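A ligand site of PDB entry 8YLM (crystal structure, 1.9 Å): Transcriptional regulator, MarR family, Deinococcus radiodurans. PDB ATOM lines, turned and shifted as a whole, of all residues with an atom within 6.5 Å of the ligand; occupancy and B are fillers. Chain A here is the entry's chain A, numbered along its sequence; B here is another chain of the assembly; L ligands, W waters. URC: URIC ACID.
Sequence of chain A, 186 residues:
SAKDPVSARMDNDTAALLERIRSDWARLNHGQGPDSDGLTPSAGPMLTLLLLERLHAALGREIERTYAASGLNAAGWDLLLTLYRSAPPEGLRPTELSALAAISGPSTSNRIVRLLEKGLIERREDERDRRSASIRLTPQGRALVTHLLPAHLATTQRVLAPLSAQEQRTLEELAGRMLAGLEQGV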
ATOM      1  N   ALA A  74      -8.109  12.883  -1.355  1.00  0.00           N
ATOM      2  CA  ALA A  74      -6.968  12.762  -0.444  1.00  0.00           C
ATOM      3  C   ALA A  74      -6.702  11.298  -0.071  1.00  0.00           C
ATOM      4  O   ALA A  74      -5.535  10.864  -0.012  1.00  0.00           O
ATOM      5  CB  ALA A  74      -7.200  13.617   0.804  1.00  0.00           C
ATOM      6  N   ALA A  75      -7.765  10.535   0.199  1.00  0.00           N
ATOM      7  CA  ALA A  75      -7.613   9.117   0.528  1.00  0.00           C
ATOM      8  C   ALA A  75      -6.934   8.347  -0.594  1.00  0.00           C
ATOM      9  O   ALA A  75      -6.083   7.485  -0.331  1.00  0.00           O
ATOM     10  CB  ALA A  75      -8.980   8.516   0.858  1.00  0.00           C
ATOM     11  N   TRP A  77      -4.923   9.537  -3.105  1.00  0.00           N
ATOM     12  CA  TRP A  77      -3.548   9.982  -3.263  1.00  0.00           C
ATOM     13  C   TRP A  77      -2.645   9.385  -2.185  1.00  0.00           C
ATOM     14  O   TRP A  77      -1.516   8.974  -2.473  1.00  0.00           O
ATOM     15  CB  TRP A  77      -3.504  11.522  -3.231  1.00  0.00           C
ATOM     16  CG  TRP A  77      -2.141  12.163  -3.326  1.00  0.00           C
ATOM     17  CD1 TRP A  77      -1.535  12.933  -2.372  1.00  0.00           C
ATOM     18  CD2 TRP A  77      -1.218  12.088  -4.421  1.00  0.00           C
ATOM     19  NE1 TRP A  77      -0.309  13.354  -2.824  1.00  0.00           N
ATOM     20  CE2 TRP A  77      -0.095  12.853  -4.076  1.00  0.00           C
ATOM     21  CE3 TRP A  77      -1.250  11.456  -5.670  1.00  0.00           C
ATOM     22  CZ2 TRP A  77       1.006  12.990  -4.927  1.00  0.00           C
ATOM     23  CZ3 TRP A  77      -0.147  11.602  -6.519  1.00  0.00           C
ATOM     24  CH2 TRP A  77       0.961  12.359  -6.133  1.00  0.00           C
ATOM     25  N   ASP A  78      -3.141   9.334  -0.953  1.00  0.00           N
ATOM     26  CA  ASP A  78      -2.423   8.704   0.149  1.00  0.00           C
ATOM     27  C   ASP A  78      -2.071   7.258  -0.159  1.00  0.00           C
ATOM     28  O   ASP A  78      -0.940   6.823   0.042  1.00  0.00           O
ATOM     29  CB  ASP A  78      -3.265   8.814   1.435  1.00  0.00           C
ATOM     30  CG  ASP A  78      -2.648   8.081   2.635  1.00  0.00           C
ATOM     31  OD1 ASP A  78      -1.420   8.144   2.841  1.00  0.00           O
ATOM     32  OD2 ASP A  78      -3.422   7.475   3.413  1.00  0.00           O
ATOM     33  N   LEU A  79      -3.052   6.490  -0.629  1.00  0.00           N
ATOM     34  CA  LEU A  79      -2.786   5.082  -0.936  1.00  0.00           C
ATOM     35  C   LEU A  79      -1.752   4.933  -2.037  1.00  0.00           C
ATOM     36  O   LEU A  79      -0.825   4.128  -1.914  1.00  0.00           O
ATOM     37  CB  LEU A  79      -4.075   4.367  -1.338  1.00  0.00           C
ATOM     38  CG  LEU A  79      -3.786   2.866  -1.149  1.00  0.00           C
ATOM     39  CD1 LEU A  79      -3.741   2.545   0.350  1.00  0.00           C
ATOM     40  CD2 LEU A  79      -4.728   1.985  -1.881  1.00  0.00           C
ATOM     41  N   LEU A  81       0.554   7.046  -3.052  1.00  0.00           N
ATOM     42  CA  LEU A  81       1.863   7.458  -2.568  1.00  0.00           C
ATOM     43  C   LEU A  81       2.446   6.438  -1.601  1.00  0.00           C
ATOM     44  O   LEU A  81       3.655   6.200  -1.591  1.00  0.00           O
ATOM     45  CB  LEU A  81       1.771   8.831  -1.894  1.00  0.00           C
ATOM     46  CG  LEU A  81       2.080  10.092  -2.670  1.00  0.00           C
ATOM     47  CD1 LEU A  81       2.326  11.192  -1.651  1.00  0.00           C
ATOM     48  CD2 LEU A  81       3.300   9.873  -3.585  1.00  0.00           C
ATOM     49  N   THR A  82       1.598   5.868  -0.749  1.00  0.00           N
ATOM     50  CA  THR A  82       2.090   4.837   0.173  1.00  0.00           C
ATOM     51  C   THR A  82       2.692   3.671  -0.587  1.00  0.00           C
ATOM     52  O   THR A  82       3.769   3.183  -0.237  1.00  0.00           O
ATOM     53  CB  THR A  82       0.953   4.378   1.098  1.00  0.00           C
ATOM     54  OG1 THR A  82       0.567   5.474   1.914  1.00  0.00           O
ATOM     55  CG2 THR A  82       1.390   3.204   2.004  1.00  0.00           C
ATOM     56  N   ARG A  85       6.222   4.756  -2.212  1.00  0.00           N
ATOM     57  CA  ARG A  85       7.392   4.888  -1.353  1.00  0.00           C
ATOM     58  C   ARG A  85       7.622   3.699  -0.435  1.00  0.00           C
ATOM     59  O   ARG A  85       8.757   3.494  -0.004  1.00  0.00           O
ATOM     60  CB  ARG A  85       7.265   6.149  -0.487  1.00  0.00           C
ATOM     61  CG  ARG A  85       5.979   6.111   0.335  1.00  0.00           C
ATOM     62  CD  ARG A  85       6.109   6.669   1.738  1.00  0.00           C
ATOM     63  NE  ARG A  85       4.813   7.189   2.209  1.00  0.00           N
ATOM     64  CZ  ARG A  85       3.979   6.518   2.996  1.00  0.00           C
ATOM     65  NH1 ARG A  85       4.291   5.296   3.417  1.00  0.00           N
ATOM     66  NH2 ARG A  85       2.829   7.087   3.378  1.00  0.00           N
ATOM     67  N   SER A  86       6.599   2.899  -0.138  1.00  0.00           N
ATOM     68  CA  SER A  86       6.728   1.907   0.907  1.00  0.00           C
ATOM     69  C   SER A  86       6.474   0.472   0.471  1.00  0.00           C
ATOM     70  O   SER A  86       6.782  -0.437   1.244  1.00  0.00           O
ATOM     71  CB  SER A  86       5.775   2.229   2.083  1.00  0.00           C
ATOM     72  OG  SER A  86       6.130   3.446   2.692  1.00  0.00           O
ATOM     73  N   LEU A 100       0.905   1.520   6.863  1.00  0.00           N
ATOM     74  CA  LEU A 100       1.939   2.394   6.335  1.00  0.00           C
ATOM     75  C   LEU A 100       1.374   3.652   5.673  1.00  0.00           C
ATOM     76  O   LEU A 100       2.148   4.558   5.327  1.00  0.00           O
ATOM     77  CB  LEU A 100       2.806   1.634   5.340  1.00  0.00           C
ATOM     78  CG  LEU A 100       3.715   0.566   5.984  1.00  0.00           C
ATOM     79  CD1 LEU A 100       4.191  -0.461   4.978  1.00  0.00           C
ATOM     80  CD2 LEU A 100       4.909   1.310   6.577  1.00  0.00           C
ATOM     81  N   ALA A 101       0.072   3.711   5.462  1.00  0.00           N
ATOM     82  CA  ALA A 101      -0.564   4.874   4.885  1.00  0.00           C
ATOM     83  C   ALA A 101      -0.664   5.989   5.912  1.00  0.00           C
ATOM     84  O   ALA A 101      -0.760   5.746   7.126  1.00  0.00           O
ATOM     85  CB  ALA A 101      -1.961   4.516   4.386  1.00  0.00           C
ATOM     86  N   ALA A 102      -0.707   7.230   5.419  1.00  0.00           N
ATOM     87  CA  ALA A 102      -0.742   8.378   6.321  1.00  0.00           C
ATOM     88  C   ALA A 102      -2.157   8.720   6.793  1.00  0.00           C
ATOM     89  O   ALA A 102      -2.306   9.353   7.834  1.00  0.00           O
ATOM     90  CB  ALA A 102      -0.129   9.607   5.664  1.00  0.00           C
ATOM     91  N   ILE A 103      -3.193   8.315   6.053  1.00  0.00           N
ATOM     92  CA  ILE A 103      -4.568   8.597   6.449  1.00  0.00           C
ATOM     93  C   ILE A 103      -5.177   7.285   6.911  1.00  0.00           C
ATOM     94  O   ILE A 103      -5.109   6.278   6.196  1.00  0.00           O
ATOM     95  CB  ILE A 103      -5.386   9.227   5.307  1.00  0.00           C
ATOM     96  CG1 ILE A 103      -4.732  10.529   4.815  1.00  0.00           C
ATOM     97  CG2 ILE A 103      -6.812   9.513   5.763  1.00  0.00           C
ATOM     98  CD1 ILE A 103      -5.379  11.102   3.527  1.00  0.00           C
ATOM     99  N   HIS A 152       3.432  18.026  -6.248  1.00  0.00           N
ATOM    100  CA  HIS A 152       3.201  17.805  -4.829  1.00  0.00           C
ATOM    101  C   HIS A 152       4.404  18.270  -4.008  1.00  0.00           C
ATOM    102  O   HIS A 152       4.250  18.991  -3.012  1.00  0.00           O
ATOM    103  CB  HIS A 152       2.900  16.331  -4.575  1.00  0.00           C
ATOM    104  CG  HIS A 152       2.496  16.012  -3.175  1.00  0.00           C
ATOM    105  ND1 HIS A 152       1.354  16.531  -2.588  1.00  0.00           N
ATOM    106  CD2 HIS A 152       3.069  15.223  -2.230  1.00  0.00           C
ATOM    107  CE1 HIS A 152       1.249  16.073  -1.355  1.00  0.00           C
ATOM    108  NE2 HIS A 152       2.270  15.278  -1.115  1.00  0.00           N
ATOM    109  N   THR A 156       4.105  21.260  -1.323  1.00  0.00           N
ATOM    110  CA  THR A 156       4.383  21.084   0.096  1.00  0.00           C
ATOM    111  C   THR A 156       5.542  21.973   0.538  1.00  0.00           C
ATOM    112  O   THR A 156       5.536  22.528   1.642  1.00  0.00           O
ATOM    113  CB  THR A 156       4.619  19.606   0.426  1.00  0.00           C
ATOM    114  OG1 THR A 156       5.735  19.119  -0.327  1.00  0.00           O
ATOM    115  CG2 THR A 156       3.393  18.794   0.059  1.00  0.00           C
ATOM    116  N   ILE B  21       8.204   6.385   7.320  1.00  0.00           N
ATOM    117  CA  ILE B  21       7.950   7.037   6.036  1.00  0.00           C
ATOM    118  C   ILE B  21       9.172   7.827   5.595  1.00  0.00           C
ATOM    119  O   ILE B  21       9.554   7.798   4.426  1.00  0.00           O
ATOM    120  CB  ILE B  21       6.695   7.919   6.139  1.00  0.00           C
ATOM    121  CG1 ILE B  21       5.475   7.058   6.421  1.00  0.00           C
ATOM    122  CG2 ILE B  21       6.505   8.728   4.854  1.00  0.00           C
ATOM    123  CD1 ILE B  21       4.180   7.857   6.545  1.00  0.00           C
ATOM    124  N   TRP B  25      11.236   7.110   2.121  1.00  0.00           N
ATOM    125  CA  TRP B  25      11.556   8.119   1.106  1.00  0.00           C
ATOM    126  C   TRP B  25      13.066   8.235   0.891  1.00  0.00           C
ATOM    127  O   TRP B  25      13.524   8.331  -0.248  1.00  0.00           O
ATOM    128  CB  TRP B  25      10.990   9.478   1.500  1.00  0.00           C
ATOM    129  CG  TRP B  25       9.552   9.691   1.143  1.00  0.00           C
ATOM    130  CD1 TRP B  25       8.509   9.856   2.008  1.00  0.00           C
ATOM    131  CD2 TRP B  25       8.986   9.747  -0.169  1.00  0.00           C
ATOM    132  NE1 TRP B  25       7.344  10.038   1.310  1.00  0.00           N
ATOM    133  CE2 TRP B  25       7.597   9.965  -0.024  1.00  0.00           C
ATOM    134  CE3 TRP B  25       9.530   9.647  -1.465  1.00  0.00           C
ATOM    135  CZ2 TRP B  25       6.740  10.070  -1.114  1.00  0.00           C
ATOM    136  CZ3 TRP B  25       8.675   9.761  -2.553  1.00  0.00           C
ATOM    137  CH2 TRP B  25       7.303   9.975  -2.369  1.00  0.00           C
ATOM    138  N   MET B  46       6.915  17.211   3.061  1.00  0.00           N
ATOM    139  CA  MET B  46       5.841  16.226   3.115  1.00  0.00           C
ATOM    140  C   MET B  46       5.627  15.703   4.543  1.00  0.00           C
ATOM    141  O   MET B  46       4.488  15.579   5.002  1.00  0.00           O
ATOM    142  CB  MET B  46       6.156  15.047   2.199  1.00  0.00           C
ATOM    143  CG  MET B  46       5.879  15.288   0.737  1.00  0.00           C
ATOM    144  SD  MET B  46       5.926  13.733  -0.157  1.00  0.00           S
ATOM    145  CE  MET B  46       7.661  13.322   0.014  1.00  0.00           C
ATOM    146  N   LEU B  47       6.722  15.397   5.243  1.00  0.00           N
ATOM    147  CA  LEU B  47       6.621  14.831   6.589  1.00  0.00           C
ATOM    148  C   LEU B  47       6.092  15.846   7.599  1.00  0.00           C
ATOM    149  O   LEU B  47       5.327  15.475   8.513  1.00  0.00           O
ATOM    150  CB  LEU B  47       7.978  14.277   7.008  1.00  0.00           C
ATOM    151  CG  LEU B  47       8.263  12.984   6.250  1.00  0.00           C
ATOM    152  CD1 LEU B  47       9.746  12.750   6.129  1.00  0.00           C
ATOM    153  CD2 LEU B  47       7.590  11.821   6.978  1.00  0.00           C
ATOM    154  N   LEU B  49       3.951  18.237   6.981  1.00  0.00           N
ATOM    155  CA  LEU B  49       2.495  18.370   6.771  1.00  0.00           C
ATOM    156  C   LEU B  49       1.756  17.093   7.165  1.00  0.00           C
ATOM    157  O   LEU B  49       0.582  17.142   7.567  1.00  0.00           O
ATOM    158  CB  LEU B  49       2.207  18.728   5.316  1.00  0.00           C
ATOM    159  CG  LEU B  49       2.761  20.062   4.815  1.00  0.00           C
ATOM    160  CD1 LEU B  49       2.404  20.248   3.347  1.00  0.00           C
ATOM    161  CD2 LEU B  49       2.227  21.226   5.608  1.00  0.00           C
ATOM    162  N   LEU B  50       2.409  15.928   7.032  1.00  0.00           N
ATOM    163  CA  LEU B  50       1.773  14.704   7.504  1.00  0.00           C
ATOM    164  C   LEU B  50       1.548  14.764   9.009  1.00  0.00           C
ATOM    165  O   LEU B  50       0.497  14.358   9.506  1.00  0.00           O
ATOM    166  CB  LEU B  50       2.647  13.507   7.141  1.00  0.00           C
ATOM    167  CG  LEU B  50       2.605  13.053   5.685  1.00  0.00           C
ATOM    168  CD1 LEU B  50       3.357  11.743   5.546  1.00  0.00           C
ATOM    169  CD2 LEU B  50       1.197  12.943   5.139  1.00  0.00           C
ATOM    170  N   GLU B  53      -1.353  17.001   9.615  1.00  0.00           N
ATOM    171  CA  GLU B  53      -2.585  16.313   9.224  1.00  0.00           C
ATOM    172  C   GLU B  53      -3.005  15.281  10.277  1.00  0.00           C
ATOM    173  O   GLU B  53      -4.193  15.170  10.620  1.00  0.00           O
ATOM    174  CB  GLU B  53      -2.386  15.646   7.859  1.00  0.00           C
ATOM    175  CG  GLU B  53      -3.639  15.295   7.122  1.00  0.00           C
ATOM    176  CD  GLU B  53      -4.425  16.524   6.681  1.00  0.00           C
ATOM    177  OE1 GLU B  53      -3.843  17.629   6.591  1.00  0.00           O
ATOM    178  OE2 GLU B  53      -5.633  16.367   6.379  1.00  0.00           O
HETATM  179  N1  URC L   1       3.727  11.729   1.480  1.00  0.00           N
HETATM  180  C2  URC L   1       3.636  10.383   1.768  1.00  0.00           C
HETATM  181  C6  URC L   1       2.652  12.617   1.434  1.00  0.00           C
HETATM  182  N3  URC L   1       2.402   9.858   2.030  1.00  0.00           N
HETATM  183  O11 URC L   1       4.618   9.660   1.782  1.00  0.00           O
HETATM  184  C4  URC L   1       1.299  10.644   2.030  1.00  0.00           C
HETATM  185  C5  URC L   1       1.394  12.021   1.741  1.00  0.00           C
HETATM  186  N9  URC L   1      -0.021  10.371   2.287  1.00  0.00           N
HETATM  187  O13 URC L   1       2.827  13.811   1.173  1.00  0.00           O
HETATM  188  N7  URC L   1       0.131  12.542   1.816  1.00  0.00           N
HETATM  189  C8  URC L   1      -0.740  11.537   2.166  1.00  0.00           C
HETATM  190  O24 URC L   1      -1.954  11.661   2.333  1.00  0.00           O
HETATM  191  O   HOH W   1       2.278  15.810   3.243  1.00  0.00           O
HETATM  192  O   HOH W   2      -3.649  12.588   0.628  1.00  0.00           O
HETATM  193  O   HOH W   3      -2.432  13.251   4.635  1.00  0.00           O
HETATM  194  O   HOH W   4      -0.909  15.152   0.911  1.00  0.00           O
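Water W2 bridges an oxygen (O24) of the ligand (2.6 Å) and the backbone carbonyl oxygen (O) of Ala 74 (2.6 Å). Water W1 lies within hydrogen-bond range of the backbone carbonyl oxygen (O) of Met 46 of chain B (2.8 Å) and an oxygen (O13) of the ligand (2.9 Å).
NH2 of Arg 85 lies within hydrogen-bond range of OG1 of Thr 82. The guanidinium group of Arg 85 lies within hydrogen-bond range of the side-chain hydroxyl of Ser 86, at 2.7 Å. The backbone carbonyl oxygen (O) of His 152 lies within hydrogen-bond range of the side-chain hydroxyl (OG1) of Thr 156 (3.1 Å). OD2 of Asp 78 is in hydrogen-bond range of N of Ile 103 (2.8 Å). The side-chain carboxylate (OD1) of Asp 78 lies within hydrogen-bond range of the backbone NH (N) of Ala 102 (2.8 Å). The backbone carbonyl oxygen (O) of Asp 78 sits at hydrogen-bond distance from the side-chain hydroxyl (OG1) of Thr 82, 2.8 Å away. The backbone carbonyl oxygen of Leu 100 sits at hydrogen-bond distance from the guanidinium group of Arg 85 (3.0 Å).
Leu 81 touches the ligand (CD1 to C6, 3.4 Å). Ala 102 touches the ligand (CB to N9, 3.5 Å). Ile 103 touches the ligand. Ile 21 of chain B touches the ligand (CG2 to O11, 3.7 Å). Leu 50 of chain B touches the ligand. Hydrophobic or aromatic side chains within 4 Å of the ligand: Leu 81, Ala 102, Ile 103, His 152, Ile 21 of chain B, Trp 25 of chain B, Met 46 of chain B and Leu 50 of chain B. Ten residues have an atom within 4 Å of the ligand: Asp 78, Leu 81, Arg 85, Ala 102, Ile 103, His 152, Ile 21 of chain B, Trp 25 of chain B, Met 46 of chain B and Leu 50 of chain B. The nearest printed residue that does not touch the ligand is Ala 74 (4.4 Å).
An oxygen (O11) of the ligand sits at hydrogen-bond distance from the indole nitrogen of Trp 25 of chain B, 2.8 Å away. The side-chain sulfur (SD) of Met 46 of chain B is in hydrogen-bond range of a nitrogen (N1) of the ligand (3.4 Å). NE2 of His 152 sits at hydrogen-bond distance from O13 of the ligand (2.8 Å). The side-chain carboxylate (OD1) of Asp 78 lies within hydrogen-bond range of a nitrogen (N9) of the ligand (2.7 Å). O11 of the ligand sits at hydrogen-bond distance from NE of Arg 85 (2.5 Å).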
